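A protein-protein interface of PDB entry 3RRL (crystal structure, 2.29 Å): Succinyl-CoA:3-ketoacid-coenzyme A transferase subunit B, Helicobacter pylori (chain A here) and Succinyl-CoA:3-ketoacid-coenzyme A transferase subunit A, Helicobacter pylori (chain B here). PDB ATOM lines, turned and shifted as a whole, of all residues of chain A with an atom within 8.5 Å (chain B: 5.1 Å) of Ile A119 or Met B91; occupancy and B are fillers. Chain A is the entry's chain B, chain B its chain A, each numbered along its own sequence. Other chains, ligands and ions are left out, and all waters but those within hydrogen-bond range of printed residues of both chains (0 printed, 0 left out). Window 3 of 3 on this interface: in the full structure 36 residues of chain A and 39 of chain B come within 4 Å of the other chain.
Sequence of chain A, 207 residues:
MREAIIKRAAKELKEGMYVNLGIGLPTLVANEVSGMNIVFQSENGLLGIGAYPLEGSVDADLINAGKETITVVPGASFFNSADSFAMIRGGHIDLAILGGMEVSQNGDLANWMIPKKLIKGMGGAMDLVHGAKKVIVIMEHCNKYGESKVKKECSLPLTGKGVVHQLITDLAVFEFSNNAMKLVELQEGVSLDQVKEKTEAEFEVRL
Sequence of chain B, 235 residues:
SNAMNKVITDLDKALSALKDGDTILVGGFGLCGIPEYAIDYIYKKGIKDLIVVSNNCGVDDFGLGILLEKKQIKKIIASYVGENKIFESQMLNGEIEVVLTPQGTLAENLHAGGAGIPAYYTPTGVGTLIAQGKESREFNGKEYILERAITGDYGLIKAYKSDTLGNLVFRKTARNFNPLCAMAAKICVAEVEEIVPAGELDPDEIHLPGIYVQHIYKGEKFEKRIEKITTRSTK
The backbone carbonyl oxygen of Lys A120 is in hydrogen-bond range of the backbone NH of Val B81 (2.9 Å).
Glu B88 touches Ile A119 (OE2 to O, 3.7 Å). Met B91 touches Ile A119 (CE to CG2, 3.5 Å). Leu B100 touches Lys A120 (CD2 to O, 3.7 Å). Leu B100 touches Gly A121. Met A122 touches Leu B100.
Ile A119 touches just these residues of chain B: Glu B88 (3.7 Å) and Met B91 (3.5 Å). Of the printed residues of chain B, Lys A120 touches Val B81 and Leu B100. Of the printed residues of chain B, Gly A121 touches Leu B100. Of the printed residues of chain A, Glu B88 touches Ile A119. Printed residues of chain A within 4 Å of Met B91: Ile A119. The nearest residue of chain A that does not touch Met B91 is Met A113 (5.9 Å). The nearest printed residue of chain A that does not touch Glu B88 is Lys A120 (5.5 Å).
Of the 12 printed residues of chain A, 4 touch a printed residue of chain B. Hydrophobic or aromatic side chains of chain A that line the printed part of chain B: Ile A119 and Met A122. Of the 13 printed residues of chain B, 4 touch a printed residue of chain A. Hydrophobic or aromatic side chains of chain B that line the printed part of chain A: Val B81, Met B91 and Leu B100.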
ATOM      1  N   TRP A 112      34.357 -28.247 -15.493  1.00  0.00           N
ATOM      2  CA  TRP A 112      33.049 -28.353 -14.869  1.00  0.00           C
ATOM      3  C   TRP A 112      31.838 -27.860 -15.649  1.00  0.00           C
ATOM      4  O   TRP A 112      30.721 -28.247 -15.354  1.00  0.00           O
ATOM      5  CB  TRP A 112      33.065 -27.674 -13.508  1.00  0.00           C
ATOM      6  CG  TRP A 112      33.185 -26.205 -13.564  1.00  0.00           C
ATOM      7  CD1 TRP A 112      34.302 -25.499 -13.797  1.00  0.00           C
ATOM      8  CD2 TRP A 112      32.147 -25.257 -13.361  1.00  0.00           C
ATOM      9  NE1 TRP A 112      34.038 -24.168 -13.763  1.00  0.00           N
ATOM     10  CE2 TRP A 112      32.715 -23.991 -13.486  1.00  0.00           C
ATOM     11  CE3 TRP A 112      30.787 -25.357 -13.082  1.00  0.00           C
ATOM     12  CZ2 TRP A 112      31.980 -22.836 -13.348  1.00  0.00           C
ATOM     13  CZ3 TRP A 112      30.061 -24.211 -12.952  1.00  0.00           C
ATOM     14  CH2 TRP A 112      30.653 -22.968 -13.085  1.00  0.00           C
ATOM     15  N   MET A 113      32.044 -26.991 -16.619  1.00  0.00           N
ATOM     16  CA  MET A 113      30.911 -26.432 -17.315  1.00  0.00           C
ATOM     17  C   MET A 113      31.079 -26.145 -18.807  1.00  0.00           C
ATOM     18  O   MET A 113      32.092 -25.624 -19.238  1.00  0.00           O
ATOM     19  CB  MET A 113      30.515 -25.150 -16.593  1.00  0.00           C
ATOM     20  CG  MET A 113      29.628 -24.229 -17.361  1.00  0.00           C
ATOM     21  SD  MET A 113      29.152 -22.711 -16.277  1.00  0.00           S
ATOM     22  CE  MET A 113      27.417 -23.322 -15.696  1.00  0.00           C
ATOM     23  N   ILE A 114      30.040 -26.450 -19.571  1.00  0.00           N
ATOM     24  CA  ILE A 114      29.892 -25.978 -20.944  1.00  0.00           C
ATOM     25  C   ILE A 114      28.611 -25.151 -21.033  1.00  0.00           C
ATOM     26  O   ILE A 114      27.518 -25.693 -20.859  1.00  0.00           O
ATOM     27  CB  ILE A 114      29.806 -27.143 -21.939  1.00  0.00           C
ATOM     28  CG1 ILE A 114      31.025 -28.059 -21.796  1.00  0.00           C
ATOM     29  CG2 ILE A 114      29.701 -26.617 -23.365  1.00  0.00           C
ATOM     30  CD1 ILE A 114      30.923 -29.344 -22.609  1.00  0.00           C
ATOM     31  N   PRO A 115      28.737 -23.844 -21.313  1.00  0.00           N
ATOM     32  CA  PRO A 115      27.599 -22.916 -21.279  1.00  0.00           C
ATOM     33  C   PRO A 115      26.388 -23.415 -22.060  1.00  0.00           C
ATOM     34  O   PRO A 115      26.528 -23.869 -23.196  1.00  0.00           O
ATOM     35  CB  PRO A 115      28.154 -21.666 -21.956  1.00  0.00           C
ATOM     36  CG  PRO A 115      29.615 -21.711 -21.674  1.00  0.00           C
ATOM     37  CD  PRO A 115      29.994 -23.166 -21.677  1.00  0.00           C
ATOM     38  N   LYS A 116      25.219 -23.351 -21.427  1.00  0.00           N
ATOM     39  CA  LYS A 116      23.939 -23.646 -22.070  1.00  0.00           C
ATOM     40  C   LYS A 116      23.925 -25.034 -22.696  1.00  0.00           C
ATOM     41  O   LYS A 116      23.101 -25.322 -23.561  1.00  0.00           O
ATOM     42  CB  LYS A 116      23.612 -22.588 -23.132  1.00  0.00           C
ATOM     43  N   LYS A 117      24.837 -25.892 -22.252  1.00  0.00           N
ATOM     44  CA  LYS A 117      24.882 -27.271 -22.717  1.00  0.00           C
ATOM     45  C   LYS A 117      25.023 -28.222 -21.543  1.00  0.00           C
ATOM     46  O   LYS A 117      24.093 -28.956 -21.199  1.00  0.00           O
ATOM     47  CB  LYS A 117      26.023 -27.473 -23.724  1.00  0.00           C
ATOM     48  N   LEU A 118      26.192 -28.183 -20.915  1.00  0.00           N
ATOM     49  CA  LEU A 118      26.490 -29.067 -19.801  1.00  0.00           C
ATOM     50  C   LEU A 118      26.613 -28.272 -18.501  1.00  0.00           C
ATOM     51  O   LEU A 118      27.615 -27.583 -18.269  1.00  0.00           O
ATOM     52  CB  LEU A 118      27.791 -29.819 -20.103  1.00  0.00           C
ATOM     53  CG  LEU A 118      28.420 -30.801 -19.117  1.00  0.00           C
ATOM     54  CD1 LEU A 118      28.907 -32.065 -19.837  1.00  0.00           C
ATOM     55  CD2 LEU A 118      29.564 -30.124 -18.386  1.00  0.00           C
ATOM     56  N   ILE A 119      25.594 -28.390 -17.651  1.00  0.00           N
ATOM     57  CA  ILE A 119      25.632 -27.797 -16.323  1.00  0.00           C
ATOM     58  C   ILE A 119      25.272 -28.830 -15.251  1.00  0.00           C
ATOM     59  O   ILE A 119      24.123 -29.258 -15.127  1.00  0.00           O
ATOM     60  CB  ILE A 119      24.718 -26.569 -16.221  1.00  0.00           C
ATOM     61  CG1 ILE A 119      24.996 -25.607 -17.380  1.00  0.00           C
ATOM     62  CG2 ILE A 119      24.957 -25.857 -14.904  1.00  0.00           C
ATOM     63  CD1 ILE A 119      24.143 -24.345 -17.374  1.00  0.00           C
ATOM     64  N   LYS A 120      26.264 -29.197 -14.455  1.00  0.00           N
ATOM     65  CA  LYS A 120      26.095 -30.208 -13.427  1.00  0.00           C
ATOM     66  C   LYS A 120      26.539 -29.574 -12.117  1.00  0.00           C
ATOM     67  O   LYS A 120      25.782 -29.499 -11.142  1.00  0.00           O
ATOM     68  CB  LYS A 120      26.935 -31.446 -13.742  1.00  0.00           C
ATOM     69  N   GLY A 121      27.801 -29.165 -12.100  1.00  0.00           N
ATOM     70  CA  GLY A 121      28.367 -28.424 -10.993  1.00  0.00           C
ATOM     71  C   GLY A 121      29.829 -28.781 -10.975  1.00  0.00           C
ATOM     72  O   GLY A 121      30.267 -29.583 -11.807  1.00  0.00           O
ATOM     73  N   MET A 122      30.588 -28.197 -10.053  1.00  0.00           N
ATOM     74  CA  MET A 122      32.008 -28.519  -9.960  1.00  0.00           C
ATOM     75  C   MET A 122      32.344 -29.615  -8.951  1.00  0.00           C
ATOM     76  O   MET A 122      33.463 -30.132  -8.956  1.00  0.00           O
ATOM     77  CB  MET A 122      32.829 -27.262  -9.650  1.00  0.00           C
ATOM     78  CG  MET A 122      32.575 -26.671  -8.261  1.00  0.00           C
ATOM     79  SD  MET A 122      30.795 -25.885  -8.101  1.00  0.00           S
ATOM     80  CE  MET A 122      30.957 -24.487  -9.448  1.00  0.00           C
ATOM     81  N   PRO A 157      34.471 -22.020 -19.010  1.00  0.00           N
ATOM     82  CA  PRO A 157      34.636 -21.521 -17.639  1.00  0.00           C
ATOM     83  C   PRO A 157      35.720 -22.305 -16.909  1.00  0.00           C
ATOM     84  O   PRO A 157      35.743 -23.540 -16.986  1.00  0.00           O
ATOM     85  CB  PRO A 157      33.270 -21.788 -17.004  1.00  0.00           C
ATOM     86  CG  PRO A 157      32.313 -21.747 -18.171  1.00  0.00           C
ATOM     87  CD  PRO A 157      33.070 -22.369 -19.311  1.00  0.00           C
ATOM     88  N   VAL B  81      24.619 -31.533  -9.373  1.00  0.00           N
ATOM     89  CA  VAL B  81      23.330 -32.194  -9.527  1.00  0.00           C
ATOM     90  C   VAL B  81      23.400 -33.370 -10.523  1.00  0.00           C
ATOM     91  O   VAL B  81      23.557 -34.520 -10.113  1.00  0.00           O
ATOM     92  CB  VAL B  81      22.223 -31.165  -9.906  1.00  0.00           C
ATOM     93  CG1 VAL B  81      22.164 -30.047  -8.875  1.00  0.00           C
ATOM     94  CG2 VAL B  81      22.471 -30.574 -11.279  1.00  0.00           C
ATOM     95  N   PHE B  87      15.016 -31.657 -12.822  1.00  0.00           N
ATOM     96  CA  PHE B  87      15.775 -30.554 -12.242  1.00  0.00           C
ATOM     97  C   PHE B  87      16.171 -29.532 -13.303  1.00  0.00           C
ATOM     98  O   PHE B  87      15.696 -28.396 -13.296  1.00  0.00           O
ATOM     99  CB  PHE B  87      17.030 -31.083 -11.542  1.00  0.00           C
ATOM    100  CG  PHE B  87      17.857 -30.013 -10.885  1.00  0.00           C
ATOM    101  CD1 PHE B  87      17.616 -29.641  -9.575  1.00  0.00           C
ATOM    102  CD2 PHE B  87      18.879 -29.385 -11.576  1.00  0.00           C
ATOM    103  CE1 PHE B  87      18.374 -28.661  -8.965  1.00  0.00           C
ATOM    104  CE2 PHE B  87      19.642 -28.403 -10.969  1.00  0.00           C
ATOM    105  CZ  PHE B  87      19.388 -28.042  -9.662  1.00  0.00           C
ATOM    106  N   GLU B  88      17.043 -29.948 -14.216  1.00  0.00           N
ATOM    107  CA  GLU B  88      17.548 -29.062 -15.260  1.00  0.00           C
ATOM    108  C   GLU B  88      16.415 -28.381 -16.019  1.00  0.00           C
ATOM    109  O   GLU B  88      16.559 -27.249 -16.478  1.00  0.00           O
ATOM    110  CB  GLU B  88      18.454 -29.836 -16.220  1.00  0.00           C
ATOM    111  CG  GLU B  88      19.665 -30.449 -15.537  1.00  0.00           C
ATOM    112  CD  GLU B  88      20.511 -31.279 -16.478  1.00  0.00           C
ATOM    113  OE1 GLU B  88      20.110 -31.439 -17.652  1.00  0.00           O
ATOM    114  OE2 GLU B  88      21.575 -31.772 -16.046  1.00  0.00           O
ATOM    115  N   SER B  89      15.290 -29.076 -16.144  1.00  0.00           N
ATOM    116  CA  SER B  89      14.118 -28.522 -16.811  1.00  0.00           C
ATOM    117  C   SER B  89      13.657 -27.244 -16.120  1.00  0.00           C
ATOM    118  O   SER B  89      13.320 -26.256 -16.774  1.00  0.00           O
ATOM    119  CB  SER B  89      12.987 -29.548 -16.826  1.00  0.00           C
ATOM    120  OG  SER B  89      13.419 -30.766 -17.408  1.00  0.00           O
ATOM    121  N   GLN B  90      13.646 -27.273 -14.793  1.00  0.00           N
ATOM    122  CA  GLN B  90      13.245 -26.119 -13.999  1.00  0.00           C
ATOM    123  C   GLN B  90      14.371 -25.097 -13.922  1.00  0.00           C
ATOM    124  O   GLN B  90      14.126 -23.903 -13.751  1.00  0.00           O
ATOM    125  CB  GLN B  90      12.839 -26.556 -12.590  1.00  0.00           C
ATOM    126  CG  GLN B  90      11.832 -27.693 -12.560  1.00  0.00           C
ATOM    127  CD  GLN B  90      11.387 -28.036 -11.152  1.00  0.00           C
ATOM    128  OE1 GLN B  90      11.615 -27.276 -10.212  1.00  0.00           O
ATOM    129  NE2 GLN B  90      10.747 -29.188 -11.000  1.00  0.00           N
ATOM    130  N   MET B  91      15.606 -25.574 -14.045  1.00  0.00           N
ATOM    131  CA  MET B  91      16.776 -24.704 -14.005  1.00  0.00           C
ATOM    132  C   MET B  91      16.833 -23.816 -15.241  1.00  0.00           C
ATOM    133  O   MET B  91      16.975 -22.597 -15.133  1.00  0.00           O
ATOM    134  CB  MET B  91      18.056 -25.534 -13.905  1.00  0.00           C
ATOM    135  CG  MET B  91      19.321 -24.708 -13.732  1.00  0.00           C
ATOM    136  SD  MET B  91      20.942 -25.799 -13.724  1.00  0.00           S
ATOM    137  CE  MET B  91      22.229 -24.436 -13.187  1.00  0.00           C
ATOM    138  N   LEU B  92      16.724 -24.437 -16.413  1.00  0.00           N
ATOM    139  CA  LEU B  92      16.727 -23.711 -17.681  1.00  0.00           C
ATOM    140  C   LEU B  92      15.557 -22.738 -17.728  1.00  0.00           C
ATOM    141  O   LEU B  92      15.737 -21.545 -17.975  1.00  0.00           O
ATOM    142  CB  LEU B  92      16.656 -24.684 -18.859  1.00  0.00           C
ATOM    143  N   ASN B  93      14.358 -23.256 -17.480  1.00  0.00           N
ATOM    144  CA  ASN B  93      13.162 -22.426 -17.405  1.00  0.00           C
ATOM    145  C   ASN B  93      13.316 -21.316 -16.369  1.00  0.00           C
ATOM    146  O   ASN B  93      12.688 -20.263 -16.474  1.00  0.00           O
ATOM    147  CB  ASN B  93      11.933 -23.279 -17.082  1.00  0.00           C
ATOM    148  N   GLY B  94      14.156 -21.561 -15.369  1.00  0.00           N
ATOM    149  CA  GLY B  94      14.426 -20.574 -14.342  1.00  0.00           C
ATOM    150  C   GLY B  94      13.415 -20.587 -13.211  1.00  0.00           C
ATOM    151  O   GLY B  94      13.361 -19.649 -12.416  1.00  0.00           O
ATOM    152  N   GLU B  95      12.615 -21.647 -13.134  1.00  0.00           N
ATOM    153  CA  GLU B  95      11.638 -21.788 -12.058  1.00  0.00           C
ATOM    154  C   GLU B  95      12.335 -22.016 -10.717  1.00  0.00           C
ATOM    155  O   GLU B  95      11.707 -21.956  -9.656  1.00  0.00           O
ATOM    156  CB  GLU B  95      10.669 -22.934 -12.357  1.00  0.00           C
ATOM    157  N   ILE B  96      13.638 -22.279 -10.776  1.00  0.00           N
ATOM    158  CA  ILE B  96      14.435 -22.477  -9.571  1.00  0.00           C
ATOM    159  C   ILE B  96      15.811 -21.834  -9.700  1.00  0.00           C
ATOM    160  O   ILE B  96      16.504 -22.007 -10.702  1.00  0.00           O
ATOM    161  CB  ILE B  96      14.605 -23.971  -9.241  1.00  0.00           C
ATOM    162  CG1 ILE B  96      15.229 -24.142  -7.861  1.00  0.00           C
ATOM    163  CG2 ILE B  96      15.453 -24.664 -10.290  1.00  0.00           C
ATOM    164  CD1 ILE B  96      15.330 -25.581  -7.427  1.00  0.00           C
ATOM    165  N   VAL B  98      19.590 -21.672  -8.883  1.00  0.00           N
ATOM    166  CA  VAL B  98      20.638 -22.590  -8.466  1.00  0.00           C
ATOM    167  C   VAL B  98      21.937 -21.849  -8.197  1.00  0.00           C
ATOM    168  O   VAL B  98      22.421 -21.094  -9.043  1.00  0.00           O
ATOM    169  CB  VAL B  98      20.900 -23.673  -9.521  1.00  0.00           C
ATOM    170  CG1 VAL B  98      21.932 -24.662  -9.007  1.00  0.00           C
ATOM    171  CG2 VAL B  98      19.602 -24.387  -9.879  1.00  0.00           C
ATOM    172  N   LEU B 100      25.652 -22.830  -7.494  1.00  0.00           N
ATOM    173  CA  LEU B 100      26.618 -23.911  -7.438  1.00  0.00           C
ATOM    174  C   LEU B 100      27.803 -23.463  -6.602  1.00  0.00           C
ATOM    175  O   LEU B 100      28.360 -22.390  -6.818  1.00  0.00           O
ATOM    176  CB  LEU B 100      27.049 -24.339  -8.841  1.00  0.00           C
ATOM    177  CG  LEU B 100      25.978 -25.106  -9.626  1.00  0.00           C
ATOM    178  CD1 LEU B 100      26.378 -25.284 -11.072  1.00  0.00           C
ATOM    179  CD2 LEU B 100      25.708 -26.451  -8.985  1.00  0.00           C
